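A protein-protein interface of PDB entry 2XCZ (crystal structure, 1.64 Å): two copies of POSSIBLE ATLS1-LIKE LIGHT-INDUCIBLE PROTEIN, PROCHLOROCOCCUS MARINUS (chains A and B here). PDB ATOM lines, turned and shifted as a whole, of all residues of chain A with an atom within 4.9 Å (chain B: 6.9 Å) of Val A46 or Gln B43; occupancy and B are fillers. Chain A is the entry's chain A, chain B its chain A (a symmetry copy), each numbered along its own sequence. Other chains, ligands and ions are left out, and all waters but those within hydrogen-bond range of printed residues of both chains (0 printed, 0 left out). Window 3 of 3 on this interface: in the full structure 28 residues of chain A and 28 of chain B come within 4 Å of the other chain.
The side-chain amide oxygen of Asn B5 lies close to the side-chain amide oxygen of Gln A7.
OE1 of Gln A7 sits at hydrogen-bond distance from OG of Ser B41, at 3.1 Å.
N of Leu B42 is in hydrogen-bond range of O of Pro A47, at 3.0 Å.
The side-chain sulfur (SD) of Met A48 lies close to the side-chain amide oxygen (OE1) of Gln A7, 3.6 Å away.
The backbone NH (N) of Val A46 sits at hydrogen-bond distance from the backbone carbonyl oxygen (O) of Ala A8, at 3.2 Å.
The side-chain amide oxygen (OD1) of Asn B5 is in hydrogen-bond range of the side-chain hydroxyl (OG) of Ser B41, 2.5 Å away.
The backbone NH (N) of Ile B6 is in hydrogen-bond range of the backbone carbonyl oxygen (O) of Ser B41 (2.9 Å).
O of Ile B6 lies within hydrogen-bond range of N of Gln B43.
The backbone carbonyl oxygen (O) of Gln B43 lies within hydrogen-bond range of the backbone NH (N) of Ala B8 (2.8 Å).
Val A46 touches Gln B43.
O of Pro A47 touches CD1 of Leu B20 (3.6 Å).
O of Pro A47 touches CA of Ser B41, 3.2 Å away.
CA of Met A48 touches O of Thr B40, at 3.2 Å.
Met A48 touches Ser B41.
Of the printed residues of chain B, Val A46 touches Gln B43.
No residue of chain B comes within 4 Å of Gly A45.
Printed residues of chain A within 4 Å of Thr B40: Met A48 (3.2 Å).
Of the printed residues of chain A, Leu B20 touches Pro A47.
Cys B44 touches none of the printed residues of chain A.
The nearest printed residue of chain B that does not touch Val A46 is Ser B41 (4.04 Å).
The nearest printed residue of chain A that does not touch Gln B43 is Pro A47 (4.6 Å).
Printed residues of chain B that touch a printed residue of chain A: Asn B5, Leu B20, Thr B40, Ser B41, Leu B42 and Gln B43.
Of the 9 printed residues of chain A, 4 touch a printed residue of chain B.
Hydrophobic or aromatic side chains of chain A within 4 Å of the printed part of chain B: Val A46, Pro A47 and Met A48.
Among the printed residues, 8 pairs touch across the chains.
Among the printed residues, no Asp or Glu carboxylate lies within 4 Å of a Lys or Arg side-chain nitrogen of the other chain.
Val A46 touches Gln B43, but with the chains exchanged Gln A43 does not touch Val B46 (8.7 Å).
Positions printed for both chains: 7, 8, 9, 43, 44, 45, 46 and 48.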
ATOM      1  N   GLN A   7     -21.599 -19.732 -16.490  1.00  0.00           N
ATOM      2  CA  GLN A   7     -21.747 -19.748 -15.039  1.00  0.00           C
ATOM      3  C   GLN A   7     -20.868 -18.615 -14.489  1.00  0.00           C
ATOM      4  O   GLN A   7     -19.636 -18.646 -14.617  1.00  0.00           O
ATOM      5  CB  GLN A   7     -21.314 -21.123 -14.532  1.00  0.00           C
ATOM      6  CG  GLN A   7     -21.182 -21.292 -13.039  1.00  0.00           C
ATOM      7  CD  GLN A   7     -20.247 -22.434 -12.699  1.00  0.00           C
ATOM      8  OE1 GLN A   7     -19.111 -22.215 -12.276  1.00  0.00           O
ATOM      9  NE2 GLN A   7     -20.706 -23.664 -12.920  1.00  0.00           N
ATOM     10  N   ALA A   8     -21.491 -17.597 -13.896  1.00  0.00           N
ATOM     11  CA  ALA A   8     -20.719 -16.405 -13.513  1.00  0.00           C
ATOM     12  C   ALA A   8     -20.883 -16.076 -12.044  1.00  0.00           C
ATOM     13  O   ALA A   8     -21.914 -16.387 -11.457  1.00  0.00           O
ATOM     14  CB  ALA A   8     -21.101 -15.200 -14.388  1.00  0.00           C
ATOM     15  N   SER A   9     -19.864 -15.440 -11.472  1.00  0.00           N
ATOM     16  CA  SER A   9     -19.865 -15.064 -10.065  1.00  0.00           C
ATOM     17  C   SER A   9     -20.592 -13.748  -9.789  1.00  0.00           C
ATOM     18  O   SER A   9     -21.047 -13.506  -8.658  1.00  0.00           O
ATOM     19  CB  SER A   9     -18.434 -14.991  -9.526  1.00  0.00           C
ATOM     20  OG  SER A   9     -17.739 -13.870 -10.058  1.00  0.00           O
ATOM     21  N   GLN A  43     -26.169 -18.378 -15.902  1.00  0.00           N
ATOM     22  CA  GLN A  43     -26.415 -18.530 -14.474  1.00  0.00           C
ATOM     23  C   GLN A  43     -25.465 -17.624 -13.701  1.00  0.00           C
ATOM     24  O   GLN A  43     -24.254 -17.887 -13.612  1.00  0.00           O
ATOM     25  CB  GLN A  43     -26.244 -19.989 -14.044  1.00  0.00           C
ATOM     26  CG  GLN A  43     -26.594 -20.253 -12.576  1.00  0.00           C
ATOM     27  CD  GLN A  43     -27.993 -19.780 -12.214  1.00  0.00           C
ATOM     28  OE1 GLN A  43     -28.955 -20.048 -12.931  1.00  0.00           O
ATOM     29  NE2 GLN A  43     -28.108 -19.068 -11.097  1.00  0.00           N
ATOM     30  N   CYS A  44     -26.016 -16.547 -13.147  1.00  0.00           N
ATOM     31  CA  CYS A  44     -25.228 -15.621 -12.343  1.00  0.00           C
ATOM     32  C   CYS A  44     -25.361 -15.922 -10.840  1.00  0.00           C
ATOM     33  O   CYS A  44     -26.125 -16.815 -10.431  1.00  0.00           O
ATOM     34  CB  CYS A  44     -25.657 -14.178 -12.633  1.00  0.00           C
ATOM     35  SG  CYS A  44     -25.239 -13.587 -14.287  1.00  0.00           S
ATOM     36  N   GLY A  45     -24.611 -15.169 -10.036  1.00  0.00           N
ATOM     37  CA  GLY A  45     -24.646 -15.271  -8.585  1.00  0.00           C
ATOM     38  C   GLY A  45     -24.079 -16.542  -7.972  1.00  0.00           C
ATOM     39  O   GLY A  45     -24.376 -16.871  -6.824  1.00  0.00           O
ATOM     40  N   VAL A  46     -23.257 -17.261  -8.729  1.00  0.00           N
ATOM     41  CA  VAL A  46     -22.658 -18.505  -8.259  1.00  0.00           C
ATOM     42  C   VAL A  46     -21.360 -18.217  -7.492  1.00  0.00           C
ATOM     43  O   VAL A  46     -20.476 -17.514  -7.995  1.00  0.00           O
ATOM     44  CB  VAL A  46     -22.329 -19.426  -9.456  1.00  0.00           C
ATOM     45  CG1 VAL A  46     -21.753 -20.757  -8.975  1.00  0.00           C
ATOM     46  CG2 VAL A  46     -23.565 -19.635 -10.318  1.00  0.00           C
ATOM     47  N   PRO A  47     -21.257 -18.715  -6.252  1.00  0.00           N
ATOM     48  CA  PRO A  47     -19.999 -18.591  -5.532  1.00  0.00           C
ATOM     49  C   PRO A  47     -18.870 -19.253  -6.324  1.00  0.00           C
ATOM     50  O   PRO A  47     -18.956 -20.444  -6.686  1.00  0.00           O
ATOM     51  CB  PRO A  47     -20.276 -19.344  -4.218  1.00  0.00           C
ATOM     52  CG  PRO A  47     -21.731 -19.167  -4.025  1.00  0.00           C
ATOM     53  CD  PRO A  47     -22.313 -19.287  -5.401  1.00  0.00           C
ATOM     54  N   MET A  48     -17.840 -18.474  -6.617  1.00  0.00           N
ATOM     55  CA  MET A  48     -16.697 -18.966  -7.392  1.00  0.00           C
ATOM     56  C   MET A  48     -15.411 -18.357  -6.874  1.00  0.00           C
ATOM     57  O   MET A  48     -15.414 -17.240  -6.340  1.00  0.00           O
ATOM     58  CB  MET A  48     -16.842 -18.569  -8.860  1.00  0.00           C
ATOM     59  CG  MET A  48     -17.986 -19.257  -9.563  1.00  0.00           C
ATOM     60  SD  MET A  48     -18.010 -18.899 -11.313  1.00  0.00           S
ATOM     61  CE  MET A  48     -16.511 -19.726 -11.867  1.00  0.00           C
ATOM     62  N   ASN B   5     -16.190 -27.699 -10.278  1.00  0.00           N
ATOM     63  CA  ASN B   5     -17.534 -27.150 -10.118  1.00  0.00           C
ATOM     64  C   ASN B   5     -18.355 -28.105  -9.255  1.00  0.00           C
ATOM     65  O   ASN B   5     -18.489 -29.282  -9.592  1.00  0.00           O
ATOM     66  CB  ASN B   5     -18.190 -26.976 -11.498  1.00  0.00           C
ATOM     67  CG  ASN B   5     -17.597 -25.836 -12.309  1.00  0.00           C
ATOM     68  OD1 ASN B   5     -17.278 -24.758 -11.783  1.00  0.00           O
ATOM     69  ND2 ASN B   5     -17.487 -26.060 -13.614  1.00  0.00           N
ATOM     70  N   ILE B   6     -18.888 -27.612  -8.136  1.00  0.00           N
ATOM     71  CA  ILE B   6     -19.672 -28.458  -7.234  1.00  0.00           C
ATOM     72  C   ILE B   6     -21.135 -28.071  -7.308  1.00  0.00           C
ATOM     73  O   ILE B   6     -21.486 -26.890  -7.240  1.00  0.00           O
ATOM     74  CB  ILE B   6     -19.179 -28.343  -5.766  1.00  0.00           C
ATOM     75  CG1 ILE B   6     -17.684 -28.702  -5.645  1.00  0.00           C
ATOM     76  CG2 ILE B   6     -19.978 -29.271  -4.853  1.00  0.00           C
ATOM     77  CD1 ILE B   6     -17.025 -28.113  -4.380  1.00  0.00           C
ATOM     78  N   GLN B   7     -21.986 -29.075  -7.451  1.00  0.00           N
ATOM     79  CA  GLN B   7     -23.434 -28.895  -7.458  1.00  0.00           C
ATOM     80  C   GLN B   7     -23.994 -29.744  -6.308  1.00  0.00           C
ATOM     81  O   GLN B   7     -23.894 -30.979  -6.321  1.00  0.00           O
ATOM     82  CB  GLN B   7     -23.960 -29.338  -8.823  1.00  0.00           C
ATOM     83  CG  GLN B   7     -25.458 -29.438  -8.978  1.00  0.00           C
ATOM     84  CD  GLN B   7     -25.828 -30.382 -10.103  1.00  0.00           C
ATOM     85  OE1 GLN B   7     -26.274 -31.505  -9.864  1.00  0.00           O
ATOM     86  NE2 GLN B   7     -25.605 -29.947 -11.342  1.00  0.00           N
ATOM     87  N   ALA B   8     -24.566 -29.092  -5.295  1.00  0.00           N
ATOM     88  CA  ALA B   8     -24.957 -29.837  -4.088  1.00  0.00           C
ATOM     89  C   ALA B   8     -26.419 -29.636  -3.752  1.00  0.00           C
ATOM     90  O   ALA B   8     -26.984 -28.596  -4.074  1.00  0.00           O
ATOM     91  CB  ALA B   8     -24.063 -29.458  -2.896  1.00  0.00           C
ATOM     92  N   SER B   9     -27.009 -30.631  -3.096  1.00  0.00           N
ATOM     93  CA  SER B   9     -28.412 -30.593  -2.709  1.00  0.00           C
ATOM     94  C   SER B   9     -28.662 -29.840  -1.403  1.00  0.00           C
ATOM     95  O   SER B   9     -29.781 -29.357  -1.159  1.00  0.00           O
ATOM     96  CB  SER B   9     -28.983 -32.010  -2.610  1.00  0.00           C
ATOM     97  OG  SER B   9     -28.458 -32.700  -1.483  1.00  0.00           O
ATOM     98  N   VAL B  10     -27.627 -29.740  -0.571  1.00  0.00           N
ATOM     99  CA  VAL B  10     -27.754 -29.093   0.750  1.00  0.00           C
ATOM    100  C   VAL B  10     -27.933 -27.576   0.621  1.00  0.00           C
ATOM    101  O   VAL B  10     -27.598 -26.986  -0.403  1.00  0.00           O
ATOM    102  CB  VAL B  10     -26.546 -29.398   1.666  1.00  0.00           C
ATOM    103  CG1 VAL B  10     -26.401 -30.891   1.904  1.00  0.00           C
ATOM    104  CG2 VAL B  10     -25.266 -28.803   1.094  1.00  0.00           C
ATOM    105  N   ALA B  12     -27.406 -23.474   0.896  1.00  0.00           N
ATOM    106  CA  ALA B  12     -26.226 -22.609   0.774  1.00  0.00           C
ATOM    107  C   ALA B  12     -25.519 -22.428   2.117  1.00  0.00           C
ATOM    108  O   ALA B  12     -26.168 -22.413   3.163  1.00  0.00           O
ATOM    109  CB  ALA B  12     -26.610 -21.282   0.182  1.00  0.00           C
ATOM    110  N   LEU B  20     -14.200 -22.869  -0.677  1.00  0.00           N
ATOM    111  CA  LEU B  20     -13.664 -22.916  -2.042  1.00  0.00           C
ATOM    112  C   LEU B  20     -12.190 -22.522  -2.090  1.00  0.00           C
ATOM    113  O   LEU B  20     -11.400 -23.130  -2.818  1.00  0.00           O
ATOM    114  CB  LEU B  20     -14.483 -22.016  -2.971  1.00  0.00           C
ATOM    115  CG  LEU B  20     -15.901 -22.515  -3.302  1.00  0.00           C
ATOM    116  CD1 LEU B  20     -16.653 -21.475  -4.129  1.00  0.00           C
ATOM    117  CD2 LEU B  20     -15.903 -23.876  -4.022  1.00  0.00           C
ATOM    118  N   THR B  40     -12.851 -22.524  -9.255  1.00  0.00           N
ATOM    119  CA  THR B  40     -13.769 -23.341  -8.451  1.00  0.00           C
ATOM    120  C   THR B  40     -15.161 -22.721  -8.422  1.00  0.00           C
ATOM    121  O   THR B  40     -15.319 -21.518  -8.634  1.00  0.00           O
ATOM    122  CB  THR B  40     -13.297 -23.531  -6.963  1.00  0.00           C
ATOM    123  OG1 THR B  40     -13.597 -22.354  -6.202  1.00  0.00           O
ATOM    124  CG2 THR B  40     -11.792 -23.837  -6.856  1.00  0.00           C
ATOM    125  N   SER B  41     -16.161 -23.549  -8.164  1.00  0.00           N
ATOM    126  CA  SER B  41     -17.510 -23.042  -7.887  1.00  0.00           C
ATOM    127  C   SER B  41     -18.295 -23.957  -6.961  1.00  0.00           C
ATOM    128  O   SER B  41     -18.017 -25.158  -6.860  1.00  0.00           O
ATOM    129  CB  SER B  41     -18.295 -22.827  -9.186  1.00  0.00           C
ATOM    130  OG  SER B  41     -18.630 -24.043  -9.807  1.00  0.00           O
ATOM    131  N   LEU B  42     -19.286 -23.366  -6.287  1.00  0.00           N
ATOM    132  CA  LEU B  42     -20.200 -24.108  -5.421  1.00  0.00           C
ATOM    133  C   LEU B  42     -21.625 -23.604  -5.604  1.00  0.00           C
ATOM    134  O   LEU B  42     -21.956 -22.458  -5.243  1.00  0.00           O
ATOM    135  CB  LEU B  42     -19.791 -23.960  -3.947  1.00  0.00           C
ATOM    136  CG  LEU B  42     -20.709 -24.625  -2.907  1.00  0.00           C
ATOM    137  CD1 LEU B  42     -20.821 -26.138  -3.121  1.00  0.00           C
ATOM    138  CD2 LEU B  42     -20.239 -24.290  -1.487  1.00  0.00           C
ATOM    139  N   GLN B  43     -22.461 -24.474  -6.162  1.00  0.00           N
ATOM    140  CA  GLN B  43     -23.884 -24.198  -6.307  1.00  0.00           C
ATOM    141  C   GLN B  43     -24.672 -25.116  -5.381  1.00  0.00           C
ATOM    142  O   GLN B  43     -24.789 -26.328  -5.625  1.00  0.00           O
ATOM    143  CB  GLN B  43     -24.330 -24.381  -7.760  1.00  0.00           C
ATOM    144  CG  GLN B  43     -25.790 -24.002  -8.019  1.00  0.00           C
ATOM    145  CD  GLN B  43     -26.118 -22.589  -7.565  1.00  0.00           C
ATOM    146  OE1 GLN B  43     -25.381 -21.647  -7.853  1.00  0.00           O
ATOM    147  NE2 GLN B  43     -27.226 -22.438  -6.846  1.00  0.00           N
ATOM    148  N   CYS B  44     -25.204 -24.536  -4.309  1.00  0.00           N
ATOM    149  CA  CYS B  44     -26.018 -25.292  -3.365  1.00  0.00           C
ATOM    150  C   CYS B  44     -27.521 -25.130  -3.657  1.00  0.00           C
ATOM    151  O   CYS B  44     -27.919 -24.370  -4.558  1.00  0.00           O
ATOM    152  CB  CYS B  44     -25.708 -24.848  -1.931  1.00  0.00           C
ATOM    153  SG  CYS B  44     -24.059 -25.294  -1.346  1.00  0.00           S
ATOM    154  N   GLY B  45     -28.335 -25.849  -2.887  1.00  0.00           N
ATOM    155  CA  GLY B  45     -29.786 -25.784  -2.978  1.00  0.00           C
ATOM    156  C   GLY B  45     -30.421 -26.355  -4.236  1.00  0.00           C
ATOM    157  O   GLY B  45     -31.565 -26.038  -4.561  1.00  0.00           O
ATOM    158  N   VAL B  46     -29.689 -27.205  -4.948  1.00  0.00           N
ATOM    159  CA  VAL B  46     -30.181 -27.812  -6.179  1.00  0.00           C
ATOM    160  C   VAL B  46     -30.975 -29.088  -5.866  1.00  0.00           C
ATOM    161  O   VAL B  46     -30.487 -29.972  -5.153  1.00  0.00           O
ATOM    162  CB  VAL B  46     -28.999 -28.183  -7.103  1.00  0.00           C
ATOM    163  CG1 VAL B  46     -29.503 -28.767  -8.422  1.00  0.00           C
ATOM    164  CG2 VAL B  46     -28.111 -26.970  -7.338  1.00  0.00           C
ATOM    165  N   MET B  48     -31.932 -32.592  -6.063  1.00  0.00           N
ATOM    166  CA  MET B  48     -31.186 -33.759  -6.542  1.00  0.00           C
ATOM    167  C   MET B  48     -31.728 -35.023  -5.910  1.00  0.00           C
ATOM    168  O   MET B  48     -32.253 -34.991  -4.789  1.00  0.00           O
ATOM    169  CB  MET B  48     -29.712 -33.641  -6.159  1.00  0.00           C
ATOM    170  CG  MET B  48     -28.989 -32.523  -6.869  1.00  0.00           C
ATOM    171  SD  MET B  48     -27.236 -32.534  -6.524  1.00  0.00           S
ATOM    172  CE  MET B  48     -26.723 -34.057  -7.332  1.00  0.00           C
